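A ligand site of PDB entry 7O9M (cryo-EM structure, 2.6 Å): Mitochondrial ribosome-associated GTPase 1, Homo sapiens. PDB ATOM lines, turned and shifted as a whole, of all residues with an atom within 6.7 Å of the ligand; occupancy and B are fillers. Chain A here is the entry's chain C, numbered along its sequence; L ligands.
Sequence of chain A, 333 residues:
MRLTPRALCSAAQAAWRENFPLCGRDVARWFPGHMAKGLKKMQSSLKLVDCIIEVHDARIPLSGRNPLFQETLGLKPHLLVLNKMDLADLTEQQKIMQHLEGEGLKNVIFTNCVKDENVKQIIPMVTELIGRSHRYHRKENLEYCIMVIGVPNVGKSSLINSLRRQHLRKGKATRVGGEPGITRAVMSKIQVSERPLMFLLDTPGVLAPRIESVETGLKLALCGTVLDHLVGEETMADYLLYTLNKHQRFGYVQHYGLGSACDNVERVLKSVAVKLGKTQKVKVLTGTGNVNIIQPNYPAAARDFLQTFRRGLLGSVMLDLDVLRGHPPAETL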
ATOM      1  N   ARG A  59     -27.199 -24.534 -10.692  1.00  0.00           N
ATOM      2  CA  ARG A  59     -27.697 -25.780 -10.134  1.00  0.00           C
ATOM      3  C   ARG A  59     -28.259 -25.575  -8.733  1.00  0.00           C
ATOM      4  O   ARG A  59     -29.304 -26.124  -8.377  1.00  0.00           O
ATOM      5  CB  ARG A  59     -26.596 -26.829 -10.116  1.00  0.00           C
ATOM      6  CG  ARG A  59     -25.968 -27.117 -11.453  1.00  0.00           C
ATOM      7  CD  ARG A  59     -24.816 -28.104 -11.315  1.00  0.00           C
ATOM      8  NE  ARG A  59     -23.659 -27.521 -10.663  1.00  0.00           N
ATOM      9  CZ  ARG A  59     -22.496 -28.139 -10.497  1.00  0.00           C
ATOM     10  NH1 ARG A  59     -22.308 -29.376 -10.917  1.00  0.00           N
ATOM     11  NH2 ARG A  59     -21.505 -27.499  -9.886  1.00  0.00           N
ATOM     12  N   ASN A  83     -23.838 -19.295 -13.269  1.00  0.00           N
ATOM     13  CA  ASN A  83     -22.992 -20.110 -14.127  1.00  0.00           C
ATOM     14  C   ASN A  83     -23.563 -21.514 -14.251  1.00  0.00           C
ATOM     15  O   ASN A  83     -24.451 -21.915 -13.490  1.00  0.00           O
ATOM     16  CB  ASN A  83     -21.564 -20.176 -13.581  1.00  0.00           C
ATOM     17  CG  ASN A  83     -20.520 -20.201 -14.677  1.00  0.00           C
ATOM     18  OD1 ASN A  83     -20.844 -20.097 -15.859  1.00  0.00           O
ATOM     19  ND2 ASN A  83     -19.265 -20.346 -14.293  1.00  0.00           N
ATOM     20  N   LYS A  84     -23.048 -22.255 -15.236  1.00  0.00           N
ATOM     21  CA  LYS A  84     -23.441 -23.647 -15.486  1.00  0.00           C
ATOM     22  C   LYS A  84     -24.930 -23.750 -15.818  1.00  0.00           C
ATOM     23  O   LYS A  84     -25.689 -24.439 -15.129  1.00  0.00           O
ATOM     24  CB  LYS A  84     -23.090 -24.546 -14.306  1.00  0.00           C
ATOM     25  CG  LYS A  84     -21.663 -24.397 -13.785  1.00  0.00           C
ATOM     26  CD  LYS A  84     -21.161 -25.699 -13.195  1.00  0.00           C
ATOM     27  CE  LYS A  84     -20.075 -25.454 -12.155  1.00  0.00           C
ATOM     28  NZ  LYS A  84     -19.131 -24.385 -12.559  1.00  0.00           N
ATOM     29  N   MET A  85     -25.359 -23.072 -16.882  1.00  0.00           N
ATOM     30  CA  MET A  85     -26.731 -23.212 -17.344  1.00  0.00           C
ATOM     31  C   MET A  85     -26.990 -24.598 -17.930  1.00  0.00           C
ATOM     32  O   MET A  85     -28.124 -25.095 -17.870  1.00  0.00           O
ATOM     33  CB  MET A  85     -27.057 -22.134 -18.381  1.00  0.00           C
ATOM     34  CG  MET A  85     -27.035 -20.713 -17.846  1.00  0.00           C
ATOM     35  SD  MET A  85     -28.310 -20.436 -16.593  1.00  0.00           S
ATOM     36  CE  MET A  85     -27.864 -18.795 -16.022  1.00  0.00           C
ATOM     37  N   ASP A  86     -25.968 -25.227 -18.513  1.00  0.00           N
ATOM     38  CA  ASP A  86     -26.161 -26.516 -19.178  1.00  0.00           C
ATOM     39  C   ASP A  86     -26.614 -27.584 -18.195  1.00  0.00           C
ATOM     40  O   ASP A  86     -27.335 -28.518 -18.567  1.00  0.00           O
ATOM     41  CB  ASP A  86     -24.878 -26.932 -19.888  1.00  0.00           C
ATOM     42  CG  ASP A  86     -23.664 -26.900 -18.966  1.00  0.00           C
ATOM     43  OD1 ASP A  86     -23.809 -26.467 -17.809  1.00  0.00           O
ATOM     44  OD2 ASP A  86     -22.570 -27.316 -19.416  1.00  0.00           O
ATOM     45  N   LEU A  87     -26.194 -27.484 -16.936  1.00  0.00           N
ATOM     46  CA  LEU A  87     -26.575 -28.495 -15.947  1.00  0.00           C
ATOM     47  C   LEU A  87     -27.975 -28.274 -15.397  1.00  0.00           C
ATOM     48  O   LEU A  87     -28.496 -29.120 -14.667  1.00  0.00           O
ATOM     49  CB  LEU A  87     -25.552 -28.526 -14.805  1.00  0.00           C
ATOM     50  CG  LEU A  87     -24.405 -29.527 -14.920  1.00  0.00           C
ATOM     51  CD1 LEU A  87     -24.938 -30.954 -14.948  1.00  0.00           C
ATOM     52  CD2 LEU A  87     -23.533 -29.249 -16.138  1.00  0.00           C
ATOM     53  N   THR A 111     -25.319 -17.277 -18.636  1.00  0.00           N
ATOM     54  CA  THR A 111     -23.888 -17.431 -18.846  1.00  0.00           C
ATOM     55  C   THR A 111     -23.534 -18.910 -18.987  1.00  0.00           C
ATOM     56  O   THR A 111     -23.876 -19.718 -18.114  1.00  0.00           O
ATOM     57  CB  THR A 111     -23.097 -16.824 -17.687  1.00  0.00           C
ATOM     58  OG1 THR A 111     -23.235 -15.391 -17.714  1.00  0.00           O
ATOM     59  CG2 THR A 111     -21.621 -17.187 -17.786  1.00  0.00           C
ATOM     60  N   ASN A 112     -22.867 -19.251 -20.091  1.00  0.00           N
ATOM     61  CA  ASN A 112     -22.258 -20.572 -20.288  1.00  0.00           C
ATOM     62  C   ASN A 112     -20.819 -20.374 -20.769  1.00  0.00           C
ATOM     63  O   ASN A 112     -20.548 -20.350 -21.974  1.00  0.00           O
ATOM     64  CB  ASN A 112     -23.066 -21.412 -21.279  1.00  0.00           C
ATOM     65  CG  ASN A 112     -24.245 -22.107 -20.627  1.00  0.00           C
ATOM     66  OD1 ASN A 112     -24.128 -22.661 -19.533  1.00  0.00           O
ATOM     67  ND2 ASN A 112     -25.397 -22.084 -21.288  1.00  0.00           N
ATOM     68  N   CYS A 113     -19.898 -20.211 -19.810  1.00  0.00           N
ATOM     69  CA  CYS A 113     -18.509 -19.934 -20.162  1.00  0.00           C
ATOM     70  C   CYS A 113     -17.838 -21.150 -20.799  1.00  0.00           C
ATOM     71  O   CYS A 113     -17.191 -21.048 -21.844  1.00  0.00           O
ATOM     72  CB  CYS A 113     -17.737 -19.476 -18.929  1.00  0.00           C
ATOM     73  SG  CYS A 113     -18.002 -20.505 -17.465  1.00  0.00           S
ATOM     74  N   VAL A 114     -17.988 -22.322 -20.172  1.00  0.00           N
ATOM     75  CA  VAL A 114     -17.362 -23.536 -20.697  1.00  0.00           C
ATOM     76  C   VAL A 114     -18.045 -23.960 -21.989  1.00  0.00           C
ATOM     77  O   VAL A 114     -17.381 -24.324 -22.966  1.00  0.00           O
ATOM     78  CB  VAL A 114     -17.378 -24.644 -19.633  1.00  0.00           C
ATOM     79  CG1 VAL A 114     -17.187 -26.009 -20.276  1.00  0.00           C
ATOM     80  CG2 VAL A 114     -16.311 -24.386 -18.588  1.00  0.00           C
ATOM     81  N   LYS A 115     -19.381 -23.924 -22.016  1.00  0.00           N
ATOM     82  CA  LYS A 115     -20.114 -24.309 -23.222  1.00  0.00           C
ATOM     83  C   LYS A 115     -19.908 -23.307 -24.345  1.00  0.00           C
ATOM     84  O   LYS A 115     -20.251 -23.598 -25.500  1.00  0.00           O
ATOM     85  CB  LYS A 115     -21.600 -24.460 -22.888  1.00  0.00           C
ATOM     86  CG  LYS A 115     -22.429 -25.169 -23.953  1.00  0.00           C
ATOM     87  CD  LYS A 115     -23.902 -25.171 -23.595  1.00  0.00           C
ATOM     88  CE  LYS A 115     -24.742 -25.727 -24.732  1.00  0.00           C
ATOM     89  NZ  LYS A 115     -26.199 -25.667 -24.426  1.00  0.00           N
ATOM     90  N   GLY A 150     -17.715 -14.499  -5.763  1.00  0.00           N
ATOM     91  CA  GLY A 150     -18.576 -15.639  -6.025  1.00  0.00           C
ATOM     92  C   GLY A 150     -18.300 -16.788  -5.079  1.00  0.00           C
ATOM     93  O   GLY A 150     -17.441 -16.705  -4.196  1.00  0.00           O
ATOM     94  N   VAL A 151     -19.063 -17.858  -5.274  1.00  0.00           N
ATOM     95  CA  VAL A 151     -18.936 -19.083  -4.489  1.00  0.00           C
ATOM     96  C   VAL A 151     -17.803 -19.913  -5.081  1.00  0.00           C
ATOM     97  O   VAL A 151     -17.570 -19.856  -6.304  1.00  0.00           O
ATOM     98  CB  VAL A 151     -20.272 -19.855  -4.458  1.00  0.00           C
ATOM     99  CG1 VAL A 151     -20.631 -20.353  -5.856  1.00  0.00           C
ATOM    100  CG2 VAL A 151     -20.237 -20.995  -3.466  1.00  0.00           C
ATOM    101  N   PRO A 152     -17.047 -20.662  -4.279  1.00  0.00           N
ATOM    102  CA  PRO A 152     -16.023 -21.540  -4.851  1.00  0.00           C
ATOM    103  C   PRO A 152     -16.641 -22.616  -5.741  1.00  0.00           C
ATOM    104  O   PRO A 152     -17.789 -23.022  -5.566  1.00  0.00           O
ATOM    105  CB  PRO A 152     -15.342 -22.152  -3.622  1.00  0.00           C
ATOM    106  CG  PRO A 152     -15.541 -21.135  -2.557  1.00  0.00           C
ATOM    107  CD  PRO A 152     -16.883 -20.515  -2.821  1.00  0.00           C
ATOM    108  N   ASN A 153     -15.845 -23.065  -6.729  1.00  0.00           N
ATOM    109  CA  ASN A 153     -16.221 -24.098  -7.685  1.00  0.00           C
ATOM    110  C   ASN A 153     -17.390 -23.685  -8.575  1.00  0.00           C
ATOM    111  O   ASN A 153     -18.198 -24.540  -8.974  1.00  0.00           O
ATOM    112  CB  ASN A 153     -16.549 -25.428  -6.982  1.00  0.00           C
ATOM    113  CG  ASN A 153     -15.326 -26.048  -6.340  1.00  0.00           C
ATOM    114  OD1 ASN A 153     -14.508 -25.362  -5.731  1.00  0.00           O
ATOM    115  ND2 ASN A 153     -15.195 -27.366  -6.462  1.00  0.00           N
ATOM    116  N   VAL A 154     -17.504 -22.395  -8.895  1.00  0.00           N
ATOM    117  CA  VAL A 154     -18.528 -21.929  -9.831  1.00  0.00           C
ATOM    118  C   VAL A 154     -17.937 -21.585 -11.189  1.00  0.00           C
ATOM    119  O   VAL A 154     -18.689 -21.325 -12.136  1.00  0.00           O
ATOM    120  CB  VAL A 154     -19.268 -20.701  -9.252  1.00  0.00           C
ATOM    121  CG1 VAL A 154     -18.376 -19.469  -9.289  1.00  0.00           C
ATOM    122  CG2 VAL A 154     -20.604 -20.474  -9.958  1.00  0.00           C
ATOM    123  N   GLY A 155     -16.614 -21.606 -11.314  1.00  0.00           N
ATOM    124  CA  GLY A 155     -15.976 -21.158 -12.550  1.00  0.00           C
ATOM    125  C   GLY A 155     -16.090 -19.667 -12.774  1.00  0.00           C
ATOM    126  O   GLY A 155     -16.277 -19.224 -13.918  1.00  0.00           O
ATOM    127  N   LYS A 156     -15.970 -18.874 -11.710  1.00  0.00           N
ATOM    128  CA  LYS A 156     -15.981 -17.419 -11.867  1.00  0.00           C
ATOM    129  C   LYS A 156     -14.695 -16.934 -12.524  1.00  0.00           C
ATOM    130  O   LYS A 156     -14.690 -15.921 -13.235  1.00  0.00           O
ATOM    131  CB  LYS A 156     -16.178 -16.747 -10.512  1.00  0.00           C
ATOM    132  CG  LYS A 156     -15.150 -17.120  -9.464  1.00  0.00           C
ATOM    133  CD  LYS A 156     -15.470 -16.482  -8.118  1.00  0.00           C
ATOM    134  CE  LYS A 156     -14.487 -16.932  -7.046  1.00  0.00           C
ATOM    135  NZ  LYS A 156     -14.625 -18.382  -6.734  1.00  0.00           N
ATOM    136  N   SER A 157     -13.586 -17.646 -12.307  1.00  0.00           N
ATOM    137  CA  SER A 157     -12.335 -17.292 -12.976  1.00  0.00           C
ATOM    138  C   SER A 157     -12.432 -17.537 -14.475  1.00  0.00           C
ATOM    139  O   SER A 157     -11.749 -16.856 -15.259  1.00  0.00           O
ATOM    140  CB  SER A 157     -11.177 -18.094 -12.370  1.00  0.00           C
ATOM    141  OG  SER A 157     -11.438 -19.492 -12.422  1.00  0.00           O
ATOM    142  N   SER A 158     -13.257 -18.485 -14.894  1.00  0.00           N
ATOM    143  CA  SER A 158     -13.475 -18.711 -16.317  1.00  0.00           C
ATOM    144  C   SER A 158     -14.142 -17.507 -16.971  1.00  0.00           C
ATOM    145  O   SER A 158     -13.854 -17.184 -18.135  1.00  0.00           O
ATOM    146  CB  SER A 158     -14.317 -19.973 -16.533  1.00  0.00           C
ATOM    147  OG  SER A 158     -14.485 -20.239 -17.919  1.00  0.00           O
ATOM    148  N   LEU A 159     -15.035 -16.831 -16.250  1.00  0.00           N
ATOM    149  CA  LEU A 159     -15.641 -15.607 -16.764  1.00  0.00           C
ATOM    150  C   LEU A 159     -14.589 -14.532 -16.988  1.00  0.00           C
ATOM    151  O   LEU A 159     -14.609 -13.837 -18.004  1.00  0.00           O
ATOM    152  CB  LEU A 159     -16.719 -15.114 -15.807  1.00  0.00           C
ATOM    153  CG  LEU A 159     -17.619 -16.172 -15.165  1.00  0.00           C
ATOM    154  CD1 LEU A 159     -18.623 -15.521 -14.224  1.00  0.00           C
ATOM    155  CD2 LEU A 159     -18.333 -16.990 -16.232  1.00  0.00           C
ATOM    156  N   ASP A 202      -8.996 -11.281 -10.356  1.00  0.00           N
ATOM    157  CA  ASP A 202      -9.653 -12.426  -9.743  1.00  0.00           C
ATOM    158  C   ASP A 202      -9.544 -12.373  -8.233  1.00  0.00           C
ATOM    159  O   ASP A 202      -8.520 -11.975  -7.677  1.00  0.00           O
ATOM    160  CB  ASP A 202      -9.043 -13.726 -10.276  1.00  0.00           C
ATOM    161  CG  ASP A 202      -9.895 -14.945  -9.938  1.00  0.00           C
ATOM    162  OD1 ASP A 202     -11.127 -14.794  -9.818  1.00  0.00           O
ATOM    163  OD2 ASP A 202      -9.332 -16.043  -9.792  1.00  0.00           O
ATOM    164  N   THR A 203     -10.620 -12.788  -7.562  1.00  0.00           N
ATOM    165  CA  THR A 203     -10.671 -12.855  -6.106  1.00  0.00           C
ATOM    166  C   THR A 203     -11.096 -14.250  -5.668  1.00  0.00           C
ATOM    167  O   THR A 203     -11.929 -14.877  -6.338  1.00  0.00           O
ATOM    168  CB  THR A 203     -11.652 -11.816  -5.531  1.00  0.00           C
ATOM    169  OG1 THR A 203     -12.994 -12.285  -5.676  1.00  0.00           O
ATOM    170  CG2 THR A 203     -11.506 -10.475  -6.239  1.00  0.00           C
ATOM    171  N   GLY A 205     -13.061 -17.231  -3.771  1.00  0.00           N
ATOM    172  CA  GLY A 205     -14.441 -17.362  -3.361  1.00  0.00           C
ATOM    173  C   GLY A 205     -14.563 -17.525  -1.849  1.00  0.00           C
ATOM    174  O   GLY A 205     -13.641 -18.000  -1.174  1.00  0.00           O
ATOM    175  N   ARG A 310     -22.387 -34.762 -12.157  1.00  0.00           N
ATOM    176  CA  ARG A 310     -21.705 -33.489 -12.381  1.00  0.00           C
ATOM    177  C   ARG A 310     -21.631 -33.190 -13.876  1.00  0.00           C
ATOM    178  O   ARG A 310     -21.772 -32.040 -14.278  1.00  0.00           O
ATOM    179  CB  ARG A 310     -20.320 -33.496 -11.713  1.00  0.00           C
ATOM    180  CG  ARG A 310     -20.351 -33.358 -10.199  1.00  0.00           C
ATOM    181  CD  ARG A 310     -18.965 -33.319  -9.580  1.00  0.00           C
ATOM    182  NE  ARG A 310     -18.991 -33.539  -8.144  1.00  0.00           N
ATOM    183  CZ  ARG A 310     -17.929 -33.516  -7.338  1.00  0.00           C
ATOM    184  NH1 ARG A 310     -16.721 -33.278  -7.816  1.00  0.00           N
ATOM    185  NH2 ARG A 310     -18.083 -33.747  -6.044  1.00  0.00           N
HETATM  186  P1  LIG L   1     -13.910 -20.993  -9.044  1.00  0.00           P
HETATM  187  O1  LIG L   1     -15.180 -20.508  -8.397  1.00  0.00           O
HETATM  188  O2  LIG L   1     -13.387 -20.096 -10.142  1.00  0.00           O
HETATM  189  O3  LIG L   1     -12.861 -21.488  -8.072  1.00  0.00           O
HETATM  190  O4  LIG L   1     -14.408 -22.315  -9.800  1.00  0.00           O
HETATM  191  P2  LIG L   1     -13.421 -23.421 -10.438  1.00  0.00           P
HETATM  192  O5  LIG L   1     -12.423 -22.730 -11.324  1.00  0.00           O
HETATM  193  O6  LIG L   1     -12.954 -24.332  -9.328  1.00  0.00           O
HETATM  194  O7  LIG L   1     -14.452 -24.230 -11.374  1.00  0.00           O
HETATM  195  C1  LIG L   1     -14.752 -25.601 -11.125  1.00  0.00           C
HETATM  196  C2  LIG L   1     -15.127 -26.307 -12.418  1.00  0.00           C
HETATM  197  O8  LIG L   1     -16.390 -25.871 -12.914  1.00  0.00           O
HETATM  198  C3  LIG L   1     -14.114 -26.042 -13.524  1.00  0.00           C
HETATM  199  O9  LIG L   1     -13.223 -27.161 -13.644  1.00  0.00           O
HETATM  200  C4  LIG L   1     -14.943 -25.807 -14.777  1.00  0.00           C
HETATM  201  O10 LIG L   1     -14.635 -26.721 -15.836  1.00  0.00           O
HETATM  202  C5  LIG L   1     -16.383 -25.981 -14.341  1.00  0.00           C
HETATM  203  N1  LIG L   1     -17.239 -24.947 -14.969  1.00  0.00           N
HETATM  204  C6  LIG L   1     -17.089 -23.614 -14.864  1.00  0.00           C
HETATM  205  N2  LIG L   1     -18.050 -22.956 -15.564  1.00  0.00           N
HETATM  206  C7  LIG L   1     -18.837 -23.877 -16.134  1.00  0.00           C
HETATM  207  C8  LIG L   1     -20.033 -23.880 -17.017  1.00  0.00           C
HETATM  208  O11 LIG L   1     -20.553 -22.806 -17.393  1.00  0.00           O
HETATM  209  N3  LIG L   1     -20.549 -25.064 -17.381  1.00  0.00           N
HETATM  210  C9  LIG L   1     -20.012 -26.231 -16.975  1.00  0.00           C
HETATM  211  N4  LIG L   1     -20.583 -27.389 -17.383  1.00  0.00           N
HETATM  212  N5  LIG L   1     -18.917 -26.311 -16.184  1.00  0.00           N
HETATM  213  C10 LIG L   1     -18.297 -25.192 -15.739  1.00  0.00           C
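The side-chain amide oxygen (OD1) of Asn 112 is in hydrogen-bond range of the backbone NH (N) of Asp 86. The backbone carbonyl oxygen of Gly 155 sits at hydrogen-bond distance from the side-chain amide nitrogen of Asn 83, 3.2 Å away. The side-chain sulfur (SG) of Cys 113 lies close to the side-chain hydroxyl (OG) of Ser 158 (3.6 Å). The backbone carbonyl oxygen of Val 154 lies within hydrogen-bond range of the side-chain amide nitrogen of Asn 83, at 2.4 Å. OD1 of Asn 83 sits at hydrogen-bond distance from SG of Cys 113, at 3.3 Å. O of Val 151 lies within hydrogen-bond range of NZ of Lys 156, 3.3 Å away. The backbone carbonyl oxygen (O) of Val 154 is in hydrogen-bond range of the side-chain amino group (NZ) of Lys 84 (3.1 Å).
The backbone NH of Lys 84 lies within hydrogen-bond range of an oxygen (O11) of the ligand. SG of Cys 113 sits at hydrogen-bond distance from N2 of the ligand (3.1 Å). N of Lys 156 is in hydrogen-bond range of O2 of the ligand, at 3.3 Å. An oxygen (O2) of the ligand sits at hydrogen-bond distance from the side-chain hydroxyl (OG) of Ser 157 (3.1 Å). The backbone NH (N) of Gly 155 lies within hydrogen-bond range of an oxygen (O4) of the ligand (2.8 Å). N of Val 154 sits at hydrogen-bond distance from O1 of the ligand, at 3.0 Å. OD1 of Asn 83 lies close to O11 of the ligand, at 3.1 Å. The side-chain carboxylate (OD2) of Asp 86 lies within hydrogen-bond range of a nitrogen (N4) of the ligand (2.8 Å). NZ of Lys 84 sits at hydrogen-bond distance from O8 of the ligand (3.1 Å). O1 of the ligand is in salt-bridge range of NZ of Lys 156, at 2.8 Å. N of Ser 157 is in hydrogen-bond range of O2 of the ligand (3.3 Å). N of Asn 153 is in hydrogen-bond range of O1 of the ligand, at 3.1 Å.
The backbone carbonyl oxygen of Val 151 sits close to an oxygen (O1) of the ligand (3.2 Å). Merely in contact with the ligand: Val 114, Pro 152 and Leu 87. Hydrophobic or aromatic side chains that line the ligand: Leu 87, Val 114 and Val 154. 13 residues have an atom within 4 Å of the ligand: Asn 83, Lys 84, Asp 86, Leu 87, Cys 113, Val 114, Val 151, Pro 152, Asn 153, Val 154, Gly 155, Lys 156 and Ser 157.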
